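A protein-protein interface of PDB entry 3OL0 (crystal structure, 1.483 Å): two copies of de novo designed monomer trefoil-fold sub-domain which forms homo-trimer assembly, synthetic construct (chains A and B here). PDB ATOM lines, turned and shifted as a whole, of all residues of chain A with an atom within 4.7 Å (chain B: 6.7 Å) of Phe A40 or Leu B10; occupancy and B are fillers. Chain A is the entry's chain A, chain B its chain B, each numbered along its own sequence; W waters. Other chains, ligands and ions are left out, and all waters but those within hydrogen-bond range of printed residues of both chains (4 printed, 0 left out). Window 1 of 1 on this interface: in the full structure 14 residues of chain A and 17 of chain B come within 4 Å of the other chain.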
ATOM      1  N   HIS A   6     -33.116  22.046  33.332  1.00  0.00           N
ATOM      2  CA  HIS A   6     -33.765  23.065  32.527  1.00  0.00           C
ATOM      3  C   HIS A   6     -32.948  23.397  31.274  1.00  0.00           C
ATOM      4  O   HIS A   6     -32.429  24.505  31.142  1.00  0.00           O
ATOM      5  CB  HIS A   6     -34.018  24.313  33.387  1.00  0.00           C
ATOM      6  CG  HIS A   6     -34.982  24.065  34.509  1.00  0.00           C
ATOM      7  ND1 HIS A   6     -34.596  23.528  35.716  1.00  0.00           N
ATOM      8  CD2 HIS A   6     -36.323  24.244  34.583  1.00  0.00           C
ATOM      9  CE1 HIS A   6     -35.658  23.402  36.498  1.00  0.00           C
ATOM     10  NE2 HIS A   6     -36.716  23.826  35.834  1.00  0.00           N
ATOM     11  N   PRO A   7     -32.845  22.440  30.343  1.00  0.00           N
ATOM     12  CA  PRO A   7     -32.048  22.683  29.133  1.00  0.00           C
ATOM     13  C   PRO A   7     -32.703  23.722  28.232  1.00  0.00           C
ATOM     14  O   PRO A   7     -33.939  23.807  28.144  1.00  0.00           O
ATOM     15  CB  PRO A   7     -32.034  21.319  28.438  1.00  0.00           C
ATOM     16  CG  PRO A   7     -33.250  20.614  28.957  1.00  0.00           C
ATOM     17  CD  PRO A   7     -33.428  21.086  30.365  1.00  0.00           C
ATOM     18  N   VAL A   8     -31.864  24.492  27.553  1.00  0.00           N
ATOM     19  CA  VAL A   8     -32.342  25.539  26.668  1.00  0.00           C
ATOM     20  C   VAL A   8     -31.735  25.415  25.276  1.00  0.00           C
ATOM     21  O   VAL A   8     -30.709  24.737  25.069  1.00  0.00           O
ATOM     22  CB  VAL A   8     -32.057  26.951  27.236  1.00  0.00           C
ATOM     23  CG1 VAL A   8     -32.865  27.184  28.512  1.00  0.00           C
ATOM     24  CG2 VAL A   8     -30.560  27.153  27.488  1.00  0.00           C
ATOM     25  N   LEU A  10     -30.445  27.715  21.812  1.00  0.00           N
ATOM     26  CA  LEU A  10     -29.878  29.003  21.437  1.00  0.00           C
ATOM     27  C   LEU A  10     -30.069  29.161  19.928  1.00  0.00           C
ATOM     28  O   LEU A  10     -29.366  28.525  19.131  1.00  0.00           O
ATOM     29  CB  LEU A  10     -28.387  29.044  21.812  1.00  0.00           C
ATOM     30  CG  LEU A  10     -28.036  28.776  23.287  1.00  0.00           C
ATOM     31  CD1 LEU A  10     -26.513  28.790  23.518  1.00  0.00           C
ATOM     32  CD2 LEU A  10     -28.695  29.807  24.155  1.00  0.00           C
ATOM     33  N   LEU A  19     -27.628  26.670  17.747  1.00  0.00           N
ATOM     34  CA  LEU A  19     -26.233  26.345  18.024  1.00  0.00           C
ATOM     35  C   LEU A  19     -26.089  24.893  18.451  1.00  0.00           C
ATOM     36  O   LEU A  19     -26.909  24.371  19.188  1.00  0.00           O
ATOM     37  CB  LEU A  19     -25.671  27.237  19.129  1.00  0.00           C
ATOM     38  CG  LEU A  19     -25.339  28.683  18.755  1.00  0.00           C
ATOM     39  CD1 LEU A  19     -24.938  29.465  19.995  1.00  0.00           C
ATOM     40  CD2 LEU A  19     -24.237  28.719  17.702  1.00  0.00           C
ATOM     41  N   ARG A  20     -25.026  24.257  17.975  1.00  0.00           N
ATOM     42  CA  ARG A  20     -24.767  22.848  18.227  1.00  0.00           C
ATOM     43  C   ARG A  20     -23.283  22.642  18.514  1.00  0.00           C
ATOM     44  O   ARG A  20     -22.435  23.133  17.770  1.00  0.00           O
ATOM     45  CB  ARG A  20     -25.165  22.075  16.962  1.00  0.00           C
ATOM     46  CG  ARG A  20     -24.800  20.628  16.946  1.00  0.00           C
ATOM     47  CD  ARG A  20     -25.582  19.925  15.845  1.00  0.00           C
ATOM     48  NE  ARG A  20     -25.131  20.276  14.498  1.00  0.00           N
ATOM     49  CZ  ARG A  20     -25.673  19.776  13.391  1.00  0.00           C
ATOM     50  NH1 ARG A  20     -26.682  18.917  13.480  1.00  0.00           N
ATOM     51  NH2 ARG A  20     -25.208  20.134  12.199  1.00  0.00           N
ATOM     52  N   ILE A  21     -22.957  21.933  19.597  1.00  0.00           N
ATOM     53  CA  ILE A  21     -21.582  21.466  19.792  1.00  0.00           C
ATOM     54  C   ILE A  21     -21.522  19.984  19.486  1.00  0.00           C
ATOM     55  O   ILE A  21     -22.258  19.175  20.059  1.00  0.00           O
ATOM     56  CB  ILE A  21     -21.024  21.700  21.215  1.00  0.00           C
ATOM     57  CG1 ILE A  21     -21.294  23.120  21.703  1.00  0.00           C
ATOM     58  CG2 ILE A  21     -19.516  21.396  21.236  1.00  0.00           C
ATOM     59  CD1 ILE A  21     -20.580  23.440  23.005  1.00  0.00           C
ATOM     60  N   ILE A  38     -28.213  20.144  20.355  1.00  0.00           N
ATOM     61  CA  ILE A  38     -28.508  21.577  20.464  1.00  0.00           C
ATOM     62  C   ILE A  38     -28.943  21.991  21.869  1.00  0.00           C
ATOM     63  O   ILE A  38     -29.191  23.158  22.125  1.00  0.00           O
ATOM     64  CB  ILE A  38     -29.559  22.068  19.433  1.00  0.00           C
ATOM     65  CG1 ILE A  38     -30.942  21.466  19.718  1.00  0.00           C
ATOM     66  CG2 ILE A  38     -29.076  21.802  18.004  1.00  0.00           C
ATOM     67  CD1 ILE A  38     -32.060  22.160  18.928  1.00  0.00           C
ATOM     68  N   GLN A  39     -29.012  21.038  22.794  1.00  0.00           N
ATOM     69  CA  GLN A  39     -29.452  21.362  24.146  1.00  0.00           C
ATOM     70  C   GLN A  39     -28.294  21.862  25.002  1.00  0.00           C
ATOM     71  O   GLN A  39     -27.221  21.236  25.042  1.00  0.00           O
ATOM     72  CB  GLN A  39     -30.150  20.156  24.788  1.00  0.00           C
ATOM     73  CG  GLN A  39     -31.422  19.818  24.028  1.00  0.00           C
ATOM     74  CD  GLN A  39     -32.271  18.761  24.685  1.00  0.00           C
ATOM     75  OE1 GLN A  39     -32.309  18.644  25.910  1.00  0.00           O
ATOM     76  NE2 GLN A  39     -32.979  17.988  23.867  1.00  0.00           N
ATOM     77  N   PHE A  40     -28.520  22.988  25.675  1.00  0.00           N
ATOM     78  CA  PHE A  40     -27.519  23.604  26.544  1.00  0.00           C
ATOM     79  C   PHE A  40     -27.993  23.752  27.971  1.00  0.00           C
ATOM     80  O   PHE A  40     -29.189  23.956  28.240  1.00  0.00           O
ATOM     81  CB  PHE A  40     -27.145  25.002  26.036  1.00  0.00           C
ATOM     82  CG  PHE A  40     -26.283  24.989  24.823  1.00  0.00           C
ATOM     83  CD1 PHE A  40     -26.848  24.892  23.561  1.00  0.00           C
ATOM     84  CD2 PHE A  40     -24.907  25.081  24.942  1.00  0.00           C
ATOM     85  CE1 PHE A  40     -26.048  24.897  22.432  1.00  0.00           C
ATOM     86  CE2 PHE A  40     -24.093  25.077  23.821  1.00  0.00           C
ATOM     87  CZ  PHE A  40     -24.665  24.987  22.565  1.00  0.00           C
ATOM     88  N   GLN A  41     -27.041  23.649  28.890  1.00  0.00           N
ATOM     89  CA  GLN A  41     -27.223  24.085  30.262  1.00  0.00           C
ATOM     90  C   GLN A  41     -26.468  25.397  30.424  1.00  0.00           C
ATOM     91  O   GLN A  41     -25.272  25.480  30.126  1.00  0.00           O
ATOM     92  CB  GLN A  41     -26.649  23.063  31.244  1.00  0.00           C
ATOM     93  CG  GLN A  41     -26.682  23.534  32.696  1.00  0.00           C
ATOM     94  CD  GLN A  41     -25.780  22.724  33.622  1.00  0.00           C
ATOM     95  OE1 GLN A  41     -24.550  22.829  33.566  1.00  0.00           O
ATOM     96  NE2 GLN A  41     -26.391  21.930  34.491  1.00  0.00           N
ATOM     97  N   ILE A  42     -27.168  26.432  30.877  1.00  0.00           N
ATOM     98  CA  ILE A  42     -26.528  27.697  31.197  1.00  0.00           C
ATOM     99  C   ILE A  42     -26.495  27.781  32.717  1.00  0.00           C
ATOM    100  O   ILE A  42     -27.526  27.636  33.375  1.00  0.00           O
ATOM    101  CB  ILE A  42     -27.307  28.897  30.626  1.00  0.00           C
ATOM    102  CG1 ILE A  42     -27.433  28.771  29.106  1.00  0.00           C
ATOM    103  CG2 ILE A  42     -26.645  30.205  31.037  1.00  0.00           C
ATOM    104  CD1 ILE A  42     -28.192  29.904  28.466  1.00  0.00           C
ATOM    105  N   VAL B   8     -21.593  33.436  32.896  1.00  0.00           N
ATOM    106  CA  VAL B   8     -22.228  32.131  32.821  1.00  0.00           C
ATOM    107  C   VAL B   8     -21.482  31.259  31.826  1.00  0.00           C
ATOM    108  O   VAL B   8     -20.721  31.756  30.991  1.00  0.00           O
ATOM    109  CB  VAL B   8     -23.717  32.227  32.428  1.00  0.00           C
ATOM    110  CG1 VAL B   8     -24.518  32.980  33.504  1.00  0.00           C
ATOM    111  CG2 VAL B   8     -23.879  32.893  31.047  1.00  0.00           C
ATOM    112  N   LEU B   9     -21.688  29.950  31.942  1.00  0.00           N
ATOM    113  CA  LEU B   9     -21.092  28.972  31.046  1.00  0.00           C
ATOM    114  C   LEU B   9     -22.202  28.351  30.210  1.00  0.00           C
ATOM    115  O   LEU B   9     -23.327  28.181  30.698  1.00  0.00           O
ATOM    116  CB  LEU B   9     -20.383  27.879  31.848  1.00  0.00           C
ATOM    117  CG  LEU B   9     -19.406  28.367  32.918  1.00  0.00           C
ATOM    118  CD1 LEU B   9     -18.716  27.173  33.559  1.00  0.00           C
ATOM    119  CD2 LEU B   9     -18.376  29.305  32.317  1.00  0.00           C
ATOM    120  N   LEU B  10     -21.887  28.028  28.957  1.00  0.00           N
ATOM    121  CA  LEU B  10     -22.848  27.433  28.027  1.00  0.00           C
ATOM    122  C   LEU B  10     -22.363  26.021  27.739  1.00  0.00           C
ATOM    123  O   LEU B  10     -21.438  25.820  26.954  1.00  0.00           O
ATOM    124  CB  LEU B  10     -22.929  28.244  26.731  1.00  0.00           C
ATOM    125  CG  LEU B  10     -23.044  29.764  26.892  1.00  0.00           C
ATOM    126  CD1 LEU B  10     -23.104  30.470  25.531  1.00  0.00           C
ATOM    127  CD2 LEU B  10     -24.247  30.102  27.721  1.00  0.00           C
ATOM    128  N   LYS B  11     -22.994  25.048  28.383  1.00  0.00           N
ATOM    129  CA  LYS B  11     -22.543  23.662  28.334  1.00  0.00           C
ATOM    130  C   LYS B  11     -23.484  22.792  27.504  1.00  0.00           C
ATOM    131  O   LYS B  11     -24.686  22.774  27.744  1.00  0.00           O
ATOM    132  CB  LYS B  11     -22.476  23.124  29.764  1.00  0.00           C
ATOM    133  CG  LYS B  11     -21.783  21.794  29.917  1.00  0.00           C
ATOM    134  CD  LYS B  11     -21.785  21.363  31.380  1.00  0.00           C
ATOM    135  CE  LYS B  11     -20.794  20.248  31.630  1.00  0.00           C
ATOM    136  NZ  LYS B  11     -20.731  19.921  33.081  1.00  0.00           N
ATOM    137  N   SER B  12     -22.931  22.065  26.540  1.00  0.00           N
ATOM    138  CA  SER B  12     -23.694  21.024  25.843  1.00  0.00           C
ATOM    139  C   SER B  12     -24.121  19.937  26.833  1.00  0.00           C
ATOM    140  O   SER B  12     -23.276  19.298  27.480  1.00  0.00           O
ATOM    141  CB  SER B  12     -22.816  20.402  24.753  1.00  0.00           C
ATOM    142  OG  SER B  12     -23.241  19.068  24.455  1.00  0.00           O
ATOM    143  N   THR B  13     -25.417  19.715  26.957  1.00  0.00           N
ATOM    144  CA  THR B  13     -25.890  18.736  27.928  1.00  0.00           C
ATOM    145  C   THR B  13     -25.502  17.312  27.537  1.00  0.00           C
ATOM    146  O   THR B  13     -25.236  16.502  28.413  1.00  0.00           O
ATOM    147  CB  THR B  13     -27.394  18.833  28.158  1.00  0.00           C
ATOM    148  OG1 THR B  13     -28.076  18.640  26.918  1.00  0.00           O
ATOM    149  CG2 THR B  13     -27.758  20.201  28.735  1.00  0.00           C
ATOM    150  N   GLN B  17     -19.362  19.473  26.787  1.00  0.00           N
ATOM    151  CA  GLN B  17     -18.449  20.507  26.306  1.00  0.00           C
ATOM    152  C   GLN B  17     -19.004  21.904  26.509  1.00  0.00           C
ATOM    153  O   GLN B  17     -20.204  22.131  26.343  1.00  0.00           O
ATOM    154  CB  GLN B  17     -18.179  20.297  24.822  1.00  0.00           C
ATOM    155  CG  GLN B  17     -17.446  19.018  24.524  1.00  0.00           C
ATOM    156  CD  GLN B  17     -17.295  18.810  23.058  1.00  0.00           C
ATOM    157  OE1 GLN B  17     -16.232  19.081  22.489  1.00  0.00           O
ATOM    158  NE2 GLN B  17     -18.354  18.342  22.419  1.00  0.00           N
ATOM    159  N   TYR B  18     -18.112  22.832  26.842  1.00  0.00           N
ATOM    160  CA  TYR B  18     -18.451  24.238  26.998  1.00  0.00           C
ATOM    161  C   TYR B  18     -18.148  24.988  25.710  1.00  0.00           C
ATOM    162  O   TYR B  18     -17.169  24.709  25.025  1.00  0.00           O
ATOM    163  CB  TYR B  18     -17.632  24.861  28.135  1.00  0.00           C
ATOM    164  CG  TYR B  18     -17.908  24.241  29.479  1.00  0.00           C
ATOM    165  CD1 TYR B  18     -17.077  23.252  29.991  1.00  0.00           C
ATOM    166  CD2 TYR B  18     -19.018  24.618  30.220  1.00  0.00           C
ATOM    167  CE1 TYR B  18     -17.341  22.670  31.220  1.00  0.00           C
ATOM    168  CE2 TYR B  18     -19.294  24.034  31.447  1.00  0.00           C
ATOM    169  CZ  TYR B  18     -18.447  23.072  31.940  1.00  0.00           C
ATOM    170  OH  TYR B  18     -18.706  22.489  33.166  1.00  0.00           O
ATOM    171  N   LEU B  19     -18.994  25.957  25.382  1.00  0.00           N
ATOM    172  CA  LEU B  19     -18.757  26.816  24.242  1.00  0.00           C
ATOM    173  C   LEU B  19     -17.590  27.749  24.543  1.00  0.00           C
ATOM    174  O   LEU B  19     -17.534  28.332  25.622  1.00  0.00           O
ATOM    175  CB  LEU B  19     -20.009  27.639  23.978  1.00  0.00           C
ATOM    176  CG  LEU B  19     -20.020  28.396  22.664  1.00  0.00           C
ATOM    177  CD1 LEU B  19     -20.017  27.439  21.506  1.00  0.00           C
ATOM    178  CD2 LEU B  19     -21.247  29.288  22.629  1.00  0.00           C
ATOM    179  N   ARG B  20     -16.687  27.888  23.580  1.00  0.00           N
ATOM    180  CA  ARG B  20     -15.504  28.723  23.721  1.00  0.00           C
ATOM    181  C   ARG B  20     -15.353  29.637  22.506  1.00  0.00           C
ATOM    182  O   ARG B  20     -15.468  29.186  21.365  1.00  0.00           O
ATOM    183  CB  ARG B  20     -14.263  27.823  23.829  1.00  0.00           C
ATOM    184  CG  ARG B  20     -12.947  28.592  23.785  1.00  0.00           C
ATOM    185  CD  ARG B  20     -11.795  27.720  24.272  1.00  0.00           C
ATOM    186  NE  ARG B  20     -11.538  26.597  23.376  1.00  0.00           N
ATOM    187  CZ  ARG B  20     -10.666  25.632  23.629  1.00  0.00           C
ATOM    188  NH1 ARG B  20      -9.987  25.648  24.775  1.00  0.00           N
ATOM    189  NH2 ARG B  20     -10.490  24.648  22.756  1.00  0.00           N
ATOM    190  N   ILE B  38     -14.373  30.483  28.023  1.00  0.00           N
ATOM    191  CA  ILE B  38     -15.737  29.945  28.030  1.00  0.00           C
ATOM    192  C   ILE B  38     -16.730  30.772  28.848  1.00  0.00           C
ATOM    193  O   ILE B  38     -17.894  30.398  28.984  1.00  0.00           O
ATOM    194  CB  ILE B  38     -15.773  28.488  28.546  1.00  0.00           C
ATOM    195  CG1 ILE B  38     -15.478  28.448  30.048  1.00  0.00           C
ATOM    196  CG2 ILE B  38     -14.841  27.619  27.740  1.00  0.00           C
ATOM    197  CD1 ILE B  38     -15.759  27.090  30.681  1.00  0.00           C
ATOM    198  N   PHE B  40     -19.237  33.781  29.582  1.00  0.00           N
ATOM    199  CA  PHE B  40     -20.107  34.671  28.810  1.00  0.00           C
ATOM    200  C   PHE B  40     -20.916  35.624  29.662  1.00  0.00           C
ATOM    201  O   PHE B  40     -21.284  35.309  30.792  1.00  0.00           O
ATOM    202  CB  PHE B  40     -21.083  33.863  27.932  1.00  0.00           C
ATOM    203  CG  PHE B  40     -20.425  33.180  26.775  1.00  0.00           C
ATOM    204  CD1 PHE B  40     -20.377  33.795  25.532  1.00  0.00           C
ATOM    205  CD2 PHE B  40     -19.831  31.936  26.926  1.00  0.00           C
ATOM    206  CE1 PHE B  40     -19.759  33.175  24.456  1.00  0.00           C
ATOM    207  CE2 PHE B  40     -19.204  31.315  25.855  1.00  0.00           C
ATOM    208  CZ  PHE B  40     -19.173  31.942  24.614  1.00  0.00           C
ATOM    209  N   ILE B  42     -24.553  37.373  29.085  1.00  0.00           N
ATOM    210  CA  ILE B  42     -25.753  37.415  28.262  1.00  0.00           C
ATOM    211  C   ILE B  42     -26.552  38.678  28.587  1.00  0.00           C
ATOM    212  O   ILE B  42     -26.890  38.918  29.747  1.00  0.00           O
ATOM    213  CB  ILE B  42     -26.630  36.188  28.528  1.00  0.00           C
ATOM    214  CG1 ILE B  42     -25.817  34.924  28.269  1.00  0.00           C
ATOM    215  CG2 ILE B  42     -27.885  36.230  27.672  1.00  0.00           C
ATOM    216  CD1 ILE B  42     -26.599  33.644  28.462  1.00  0.00           C
HETATM  217  O   HOH W   1     -26.465  18.747  23.956  1.00  0.00           O
HETATM  218  O   HOH W   2     -23.358  25.320  32.455  1.00  0.00           O
HETATM  219  O   HOH W   3     -23.954  18.840  22.091  1.00  0.00           O
HETATM  220  O   HOH W   4     -30.422  17.958  27.638  1.00  0.00           O
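Phe A40 touches Leu B10, but with the chains exchanged Leu A10 does not touch Phe B40 (8.1 Å). Ile A42 touches Val B8, but with the chains exchanged Val A8 does not touch Ile B42 (7.7 Å). Ile A42 touches Leu B10, but with the chains exchanged Leu A10 does not touch Ile B42 (6.1 Å). Of the 16 pairs that touch across the chains among the printed residues, none has its exchanged pair printed and touching as well.
Ile A21 touches Gln B17 (CG2 to NE2, 3.5 Å). Tyr B18 touches Ile A21 (C to CD1, 3.95 Å). Ile A21 touches Leu B19 (CD1 to N, 3.8 Å). Phe A40 touches Leu B10 (CD2 to C, 3.9 Å). Phe A40 touches Lys B11 (CA to O, 3.2 Å). Ser B12 touches Phe A40. Phe A40 touches Thr B13 (C to CG2, 3.6 Å). Ile A42 touches Val B8. CA of Ile A42 touches O of Leu B9 (3.3 Å). Ile A42 touches Leu B10.
Of the 12 printed residues of chain A, 5 touch a printed residue of chain B. Among the printed residues, no Asp or Glu carboxylate lies within 4 Å of a Lys or Arg side-chain nitrogen of the other chain.
O of Gln A39 is in hydrogen-bond range of N of Thr B13 (3.0 Å). O of Lys B11 is in hydrogen-bond range of N of Gln A41 (2.8 Å). O of Gln A41 lies close to O of Leu B9, at 3.4 Å.
The backbone NH (N) of Val A8 sits at hydrogen-bond distance from the backbone carbonyl oxygen (O) of Phe A40. The backbone NH (N) of Val B8 is in hydrogen-bond range of the backbone carbonyl oxygen (O) of Phe B40 (2.8 Å). The backbone carbonyl oxygen of Leu B10 is in hydrogen-bond range of the backbone NH of Leu B19 (2.9 Å). The side-chain hydroxyl (OH) of Tyr B18 is in hydrogen-bond range of the side-chain amino group (NZ) of Lys B11 (3.3 Å). The backbone NH (N) of Ser B12 sits at hydrogen-bond distance from the backbone carbonyl oxygen (O) of Gln B17.
Printed residues of chain B within 4 Å of Phe A40: Leu B10, Lys B11, Ser B12 and Thr B13. Leu B10 touches just these residues of chain A: Phe A40 (3.9 Å), Gln A41 (3.8 Å) and Ile A42 (3.7 Å). Of the printed residues of chain A, Ser B12 touches Gln A39 and Phe A40. Of the printed residues of chain A, Tyr B18 touches Ile A21 (3.95 Å). Printed residues of chain B within 4 Å of Gln A41: Leu B9 (3.4 Å), Leu B10 (3.8 Å), Lys B11 (2.8 Å) and Thr B13 (3.5 Å). Of the printed residues of chain A, Thr B13 touches Gln A39 (3.0 Å), Phe A40 (3.6 Å) and Gln A41 (3.5 Å). Of the printed residues of chain A, Lys B11 touches Phe A40 (3.2 Å) and Gln A41 (2.8 Å). Leu A19 touches none of the printed residues of chain B. The nearest residue of chain A that does not touch Leu B10 is Leu A10 (4.3 Å).
Water W3 bridges the side-chain hydroxyl of Ser B12 (2.5 Å) and the backbone carbonyl oxygen of Ile A21 (2.7 Å). Water W4 bridges the side-chain hydroxyl of Thr B13 (2.5 Å) and the side-chain amide oxygen of Gln A39 (2.6 Å). Water W1 lies within hydrogen-bond range of the backbone carbonyl oxygen of Gln A39 (2.8 Å), the side-chain hydroxyl of Ser B12 (3.3 Å) and the backbone NH of Thr B13 (3.3 Å). Water W2 bridges the side-chain amide oxygen (OE1) of Gln A41 and the backbone carbonyl oxygen (O) of Leu B9.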
